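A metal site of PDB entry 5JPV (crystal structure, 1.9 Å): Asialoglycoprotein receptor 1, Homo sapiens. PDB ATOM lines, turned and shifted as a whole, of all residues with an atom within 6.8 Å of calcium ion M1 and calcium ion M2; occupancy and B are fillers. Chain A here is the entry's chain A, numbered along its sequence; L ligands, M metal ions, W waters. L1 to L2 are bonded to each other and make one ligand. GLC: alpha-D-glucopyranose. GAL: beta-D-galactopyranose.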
ATOM      1  N   ASP A  70       3.367   9.052 -29.614  1.00  0.00           N
ATOM      2  CA  ASP A  70       3.505   8.047 -30.687  1.00  0.00           C
ATOM      3  C   ASP A  70       3.963   6.689 -30.136  1.00  0.00           C
ATOM      4  O   ASP A  70       4.711   5.952 -30.797  1.00  0.00           O
ATOM      5  CB  ASP A  70       4.450   8.550 -31.788  1.00  0.00           C
ATOM      6  CG  ASP A  70       5.931   8.416 -31.434  1.00  0.00           C
ATOM      7  OD1 ASP A  70       6.306   8.460 -30.246  1.00  0.00           O
ATOM      8  OD2 ASP A  70       6.723   8.245 -32.366  1.00  0.00           O
ATOM      9  N   GLN A  71       3.484   6.366 -28.941  1.00  0.00           N
ATOM     10  CA  GLN A  71       3.844   5.107 -28.279  1.00  0.00           C
ATOM     11  C   GLN A  71       3.377   3.883 -29.069  1.00  0.00           C
ATOM     12  O   GLN A  71       3.984   2.816 -28.981  1.00  0.00           O
ATOM     13  CB  GLN A  71       3.266   5.051 -26.862  1.00  0.00           C
ATOM     14  CG  GLN A  71       3.745   6.168 -25.959  1.00  0.00           C
ATOM     15  CD  GLN A  71       3.140   6.095 -24.574  1.00  0.00           C
ATOM     16  OE1 GLN A  71       2.120   6.721 -24.296  1.00  0.00           O
ATOM     17  NE2 GLN A  71       3.772   5.342 -23.694  1.00  0.00           N
ATOM     18  N   GLY A  73       2.805   3.882 -32.503  1.00  0.00           N
ATOM     19  CA  GLY A  73       3.168   3.997 -33.903  1.00  0.00           C
ATOM     20  C   GLY A  73       3.162   5.445 -34.369  1.00  0.00           C
ATOM     21  O   GLY A  73       4.145   6.154 -34.192  1.00  0.00           O
ATOM     22  N   TRP A  75       1.972   9.513 -34.527  1.00  0.00           N
ATOM     23  CA  TRP A  75       1.557  10.568 -33.600  1.00  0.00           C
ATOM     24  C   TRP A  75       0.034  10.592 -33.456  1.00  0.00           C
ATOM     25  O   TRP A  75      -0.666  10.556 -34.460  1.00  0.00           O
ATOM     26  CB  TRP A  75       2.083  11.924 -34.063  1.00  0.00           C
ATOM     27  CG  TRP A  75       3.533  12.073 -33.804  1.00  0.00           C
ATOM     28  CD1 TRP A  75       4.550  12.066 -34.729  1.00  0.00           C
ATOM     29  CD2 TRP A  75       4.159  12.219 -32.529  1.00  0.00           C
ATOM     30  NE1 TRP A  75       5.755  12.208 -34.101  1.00  0.00           N
ATOM     31  CE2 TRP A  75       5.554  12.293 -32.752  1.00  0.00           C
ATOM     32  CE3 TRP A  75       3.677  12.287 -31.217  1.00  0.00           C
ATOM     33  CZ2 TRP A  75       6.475  12.442 -31.699  1.00  0.00           C
ATOM     34  CZ3 TRP A  75       4.596  12.435 -30.174  1.00  0.00           C
ATOM     35  CH2 TRP A  75       5.972  12.501 -30.423  1.00  0.00           C
ATOM     36  N   GLU A  93      14.099  20.973 -35.384  1.00  0.00           N
ATOM     37  CA  GLU A  93      14.848  19.734 -35.162  1.00  0.00           C
ATOM     38  C   GLU A  93      14.116  18.701 -34.281  1.00  0.00           C
ATOM     39  O   GLU A  93      14.685  17.667 -33.933  1.00  0.00           O
ATOM     40  CB  GLU A  93      16.275  20.006 -34.664  1.00  0.00           C
ATOM     41  CG  GLU A  93      17.136  20.762 -35.688  1.00  0.00           C
ATOM     42  CD  GLU A  93      18.630  20.628 -35.420  1.00  0.00           C
ATOM     43  OE1 GLU A  93      19.341  20.077 -36.299  1.00  0.00           O
ATOM     44  OE2 GLU A  93      19.090  21.041 -34.335  1.00  0.00           O
ATOM     45  N   GLN A  94      12.868  18.993 -33.953  1.00  0.00           N
ATOM     46  CA  GLN A  94      11.975  18.050 -33.248  1.00  0.00           C
ATOM     47  C   GLN A  94      10.750  17.751 -34.120  1.00  0.00           C
ATOM     48  O   GLN A  94      10.407  18.560 -34.983  1.00  0.00           O
ATOM     49  CB  GLN A  94      11.530  18.614 -31.891  1.00  0.00           C
ATOM     50  CG  GLN A  94      12.672  19.091 -30.957  1.00  0.00           C
ATOM     51  CD  GLN A  94      13.649  17.990 -30.568  1.00  0.00           C
ATOM     52  OE1 GLN A  94      13.343  16.810 -30.638  1.00  0.00           O
ATOM     53  NE2 GLN A  94      14.837  18.400 -30.116  1.00  0.00           N
ATOM     54  N   PRO A  95      10.105  16.577 -33.932  1.00  0.00           N
ATOM     55  CA  PRO A  95      10.492  15.454 -33.064  1.00  0.00           C
ATOM     56  C   PRO A  95      11.654  14.674 -33.679  1.00  0.00           C
ATOM     57  O   PRO A  95      11.791  14.652 -34.904  1.00  0.00           O
ATOM     58  CB  PRO A  95       9.229  14.579 -33.010  1.00  0.00           C
ATOM     59  CG  PRO A  95       8.483  14.902 -34.278  1.00  0.00           C
ATOM     60  CD  PRO A  95       8.856  16.311 -34.661  1.00  0.00           C
ATOM     61  N   ASP A  96      12.487  14.073 -32.847  1.00  0.00           N
ATOM     62  CA  ASP A  96      13.667  13.372 -33.358  1.00  0.00           C
ATOM     63  C   ASP A  96      13.819  11.939 -32.838  1.00  0.00           C
ATOM     64  O   ASP A  96      14.794  11.276 -33.173  1.00  0.00           O
ATOM     65  CB  ASP A  96      14.929  14.186 -33.056  1.00  0.00           C
ATOM     66  CG  ASP A  96      15.208  14.331 -31.560  1.00  0.00           C
ATOM     67  OD1 ASP A  96      14.330  13.950 -30.757  1.00  0.00           O
ATOM     68  OD2 ASP A  96      16.294  14.837 -31.204  1.00  0.00           O
ATOM     69  N   ASP A  97      12.877  11.485 -32.008  1.00  0.00           N
ATOM     70  CA  ASP A  97      12.910  10.128 -31.420  1.00  0.00           C
ATOM     71  C   ASP A  97      14.301   9.738 -30.892  1.00  0.00           C
ATOM     72  O   ASP A  97      14.830   8.675 -31.236  1.00  0.00           O
ATOM     73  CB  ASP A  97      12.423   9.093 -32.453  1.00  0.00           C
ATOM     74  CG  ASP A  97      12.014   7.763 -31.830  1.00  0.00           C
ATOM     75  OD1 ASP A  97      11.310   7.745 -30.792  1.00  0.00           O
ATOM     76  OD2 ASP A  97      12.364   6.710 -32.423  1.00  0.00           O
ATOM     77  N   TRP A  98      14.887  10.598 -30.059  1.00  0.00           N
ATOM     78  CA  TRP A  98      16.280  10.424 -29.649  1.00  0.00           C
ATOM     79  C   TRP A  98      16.468   9.196 -28.753  1.00  0.00           C
ATOM     80  O   TRP A  98      15.716   9.004 -27.815  1.00  0.00           O
ATOM     81  CB  TRP A  98      16.755  11.703 -28.955  1.00  0.00           C
ATOM     82  CG  TRP A  98      18.204  11.790 -28.568  1.00  0.00           C
ATOM     83  CD1 TRP A  98      19.299  11.570 -29.360  1.00  0.00           C
ATOM     84  CD2 TRP A  98      18.712  12.166 -27.288  1.00  0.00           C
ATOM     85  NE1 TRP A  98      20.455  11.775 -28.642  1.00  0.00           N
ATOM     86  CE2 TRP A  98      20.124  12.152 -27.371  1.00  0.00           C
ATOM     87  CE3 TRP A  98      18.103  12.529 -26.076  1.00  0.00           C
ATOM     88  CZ2 TRP A  98      20.944  12.459 -26.280  1.00  0.00           C
ATOM     89  CZ3 TRP A  98      18.916  12.843 -24.985  1.00  0.00           C
ATOM     90  CH2 TRP A  98      20.331  12.802 -25.095  1.00  0.00           C
ATOM     91  N   GLY A 106      13.293   5.235 -27.804  1.00  0.00           N
ATOM     92  CA  GLY A 106      13.502   6.594 -28.302  1.00  0.00           C
ATOM     93  C   GLY A 106      12.766   7.587 -27.406  1.00  0.00           C
ATOM     94  O   GLY A 106      12.976   7.609 -26.183  1.00  0.00           O
ATOM     95  N   GLU A 107      11.895   8.385 -28.023  1.00  0.00           N
ATOM     96  CA  GLU A 107      11.145   9.407 -27.307  1.00  0.00           C
ATOM     97  C   GLU A 107       9.726   9.401 -27.851  1.00  0.00           C
ATOM     98  O   GLU A 107       9.527   9.558 -29.051  1.00  0.00           O
ATOM     99  CB  GLU A 107      11.800  10.773 -27.474  1.00  0.00           C
ATOM    100  CG  GLU A 107      13.126  10.915 -26.713  1.00  0.00           C
ATOM    101  CD  GLU A 107      13.787  12.274 -26.922  1.00  0.00           C
ATOM    102  OE1 GLU A 107      14.421  12.779 -25.961  1.00  0.00           O
ATOM    103  OE2 GLU A 107      13.674  12.830 -28.034  1.00  0.00           O
ATOM    104  N   ASP A 108       8.746   9.177 -26.978  1.00  0.00           N
ATOM    105  CA  ASP A 108       7.402   8.907 -27.460  1.00  0.00           C
ATOM    106  C   ASP A 108       6.312   9.877 -26.981  1.00  0.00           C
ATOM    107  O   ASP A 108       5.157   9.716 -27.355  1.00  0.00           O
ATOM    108  CB  ASP A 108       6.999   7.464 -27.126  1.00  0.00           C
ATOM    109  CG  ASP A 108       7.803   6.412 -27.908  1.00  0.00           C
ATOM    110  OD1 ASP A 108       8.651   6.789 -28.757  1.00  0.00           O
ATOM    111  OD2 ASP A 108       7.573   5.211 -27.667  1.00  0.00           O
ATOM    112  N   CYS A 109       6.663  10.864 -26.172  1.00  0.00           N
ATOM    113  CA  CYS A 109       5.653  11.711 -25.537  1.00  0.00           C
ATOM    114  C   CYS A 109       6.005  13.188 -25.713  1.00  0.00           C
ATOM    115  O   CYS A 109       7.148  13.577 -25.498  1.00  0.00           O
ATOM    116  CB  CYS A 109       5.528  11.352 -24.048  1.00  0.00           C
ATOM    117  SG  CYS A 109       4.782   9.700 -23.710  1.00  0.00           S
ATOM    118  N   HIS A 111       5.944  17.309 -25.033  1.00  0.00           N
ATOM    119  CA  HIS A 111       5.769  18.349 -24.023  1.00  0.00           C
ATOM    120  C   HIS A 111       6.110  19.722 -24.580  1.00  0.00           C
ATOM    121  O   HIS A 111       6.905  19.842 -25.501  1.00  0.00           O
ATOM    122  CB  HIS A 111       6.626  18.061 -22.773  1.00  0.00           C
ATOM    123  CG  HIS A 111       8.104  18.077 -23.031  1.00  0.00           C
ATOM    124  ND1 HIS A 111       8.915  19.150 -22.689  1.00  0.00           N
ATOM    125  CD2 HIS A 111       8.919  17.143 -23.580  1.00  0.00           C
ATOM    126  CE1 HIS A 111      10.167  18.863 -23.029  1.00  0.00           C
ATOM    127  NE2 HIS A 111      10.197  17.658 -23.562  1.00  0.00           N
ATOM    128  N   ASN A 119       8.661  19.380 -27.871  1.00  0.00           N
ATOM    129  CA  ASN A 119       9.707  18.389 -27.995  1.00  0.00           C
ATOM    130  C   ASN A 119       9.127  17.001 -27.670  1.00  0.00           C
ATOM    131  O   ASN A 119       8.237  16.910 -26.821  1.00  0.00           O
ATOM    132  CB  ASN A 119      10.830  18.693 -27.011  1.00  0.00           C
ATOM    133  CG  ASN A 119      11.894  17.632 -27.020  1.00  0.00           C
ATOM    134  OD1 ASN A 119      12.307  17.181 -28.072  1.00  0.00           O
ATOM    135  ND2 ASN A 119      12.334  17.204 -25.829  1.00  0.00           N
ATOM    136  N   ASP A 120       9.621  15.961 -28.335  1.00  0.00           N
ATOM    137  CA  ASP A 120       9.324  14.592 -27.922  1.00  0.00           C
ATOM    138  C   ASP A 120      10.353  14.138 -26.898  1.00  0.00           C
ATOM    139  O   ASP A 120      11.545  14.403 -27.051  1.00  0.00           O
ATOM    140  CB  ASP A 120       9.229  13.611 -29.112  1.00  0.00           C
ATOM    141  CG  ASP A 120      10.503  13.533 -29.956  1.00  0.00           C
ATOM    142  OD1 ASP A 120      11.261  14.516 -30.053  1.00  0.00           O
ATOM    143  OD2 ASP A 120      10.723  12.467 -30.554  1.00  0.00           O
ATOM    144  N   ASP A 121       9.898  13.495 -25.838  1.00  0.00           N
ATOM    145  CA  ASP A 121      10.790  13.112 -24.762  1.00  0.00           C
ATOM    146  C   ASP A 121      10.424  11.741 -24.221  1.00  0.00           C
ATOM    147  O   ASP A 121       9.438  11.136 -24.648  1.00  0.00           O
ATOM    148  CB  ASP A 121      10.768  14.158 -23.636  1.00  0.00           C
ATOM    149  CG  ASP A 121      12.108  14.286 -22.916  1.00  0.00           C
ATOM    150  OD1 ASP A 121      12.467  15.419 -22.512  1.00  0.00           O
ATOM    151  OD2 ASP A 121      12.830  13.274 -22.777  1.00  0.00           O
HETATM  152  C1  GLC L   1      19.071  22.987 -26.140  1.00  0.00           C
HETATM  153  C2  GLC L   1      19.244  22.265 -27.486  1.00  0.00           C
HETATM  154  C3  GLC L   1      18.153  21.207 -27.706  1.00  0.00           C
HETATM  155  C4  GLC L   1      18.057  20.216 -26.547  1.00  0.00           C
HETATM  156  C5  GLC L   1      18.045  20.939 -25.190  1.00  0.00           C
HETATM  157  C6  GLC L   1      18.385  19.943 -24.090  1.00  0.00           C
HETATM  158  O1  GLC L   1      17.876  23.808 -26.160  1.00  0.00           O
HETATM  159  O2  GLC L   1      19.206  23.210 -28.568  1.00  0.00           O
HETATM  160  O3  GLC L   1      18.404  20.483 -28.910  1.00  0.00           O
HETATM  161  O4  GLC L   1      16.853  19.438 -26.763  1.00  0.00           O
HETATM  162  O5  GLC L   1      19.032  22.015 -25.058  1.00  0.00           O
HETATM  163  O6  GLC L   1      17.493  20.151 -23.002  1.00  0.00           O
HETATM  164  C1  GAL L   2      17.063  18.025 -26.611  1.00  0.00           C
HETATM  165  C2  GAL L   2      15.672  17.427 -26.414  1.00  0.00           C
HETATM  166  C3  GAL L   2      15.717  15.889 -26.466  1.00  0.00           C
HETATM  167  C4  GAL L   2      16.468  15.400 -27.719  1.00  0.00           C
HETATM  168  C5  GAL L   2      17.848  16.061 -27.771  1.00  0.00           C
HETATM  169  C6  GAL L   2      18.692  15.647 -28.974  1.00  0.00           C
HETATM  170  O2  GAL L   2      15.165  17.861 -25.144  1.00  0.00           O
HETATM  171  O3  GAL L   2      14.368  15.385 -26.473  1.00  0.00           O
HETATM  172  O4  GAL L   2      15.692  15.749 -28.872  1.00  0.00           O
HETATM  173  O5  GAL L   2      17.714  17.513 -27.789  1.00  0.00           O
HETATM  174  O6  GAL L   2      20.017  16.124 -28.760  1.00  0.00           O
HETATM  175 CA    CA M   1       8.925   8.154 -30.941  1.00  0.00          CA
HETATM  176 CA    CA M   2      13.304  15.002 -28.791  1.00  0.00          CA
HETATM  177  O   HOH W   1       9.319  10.452 -31.783  1.00  0.00           O
HETATM  178  O   HOH W   2       9.472   7.877 -33.477  1.00  0.00           O
HETATM  179  O   HOH W   3       8.701   5.827 -31.671  1.00  0.00           O
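The backbone NH (N) of Trp 98 lies close to the side-chain carboxylate (OE2) of Glu 107. N of Asp 97 lies within hydrogen-bond range of OD2 of Asp 120 (2.8 Å). The backbone NH (N) of Trp 98 sits close to the side-chain carboxylate (OD1) of Asp 96, 3.5 Å away. N of His 111 lies within hydrogen-bond range of O of Asn 119 (2.9 Å). The backbone NH (N) of Asp 108 sits at hydrogen-bond distance from the backbone carbonyl oxygen (O) of Asp 121 (3.1 Å).
Four residues have an atom within 4 Å of calcium ion M1: Asp 70, Asp 97, Glu 107 and Asp 108. The nearest printed residue that does not touch calcium ion M1 is Asp 120 (4.7 Å).
Five residues have an atom within 4 Å of calcium ion M2: Gln 94, Asp 96, Glu 107, Asn 119 and Asp 120.
Calcium ion M1 is bound by OD1 of Asp 97, 2.4 Å away. O of Glu 107 is bound to calcium ion M1, at 2.4 Å. Water W3 binds calcium ion M1 (2.4 Å). Water W1 is bound to calcium ion M1, at 2.5 Å. OD1 of Asp 108 is bound to calcium ion M1. Calcium ion M1 is bound by water W2 (2.6 Å). OD2 of Asp 70 is bound to calcium ion M1 (2.6 Å). Calcium ion M1 is bound by OD1 of Asp 70, 2.7 Å away.
Calcium ion M2 is bound by OE2 of Glu 107 (2.3 Å), OD1 of Asp 120 (2.5 Å), OD1 of Asp 96 (2.5 Å), OD1 of Asn 119 (2.5 Å), O4 of GAL L2 (2.5 Å), O of Asp 120 (2.5 Å), O3 of GAL L2 (2.6 Å) and OE1 of Gln 94 (2.6 Å). Calcium ion M2 has eight donor atoms within binding distance.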
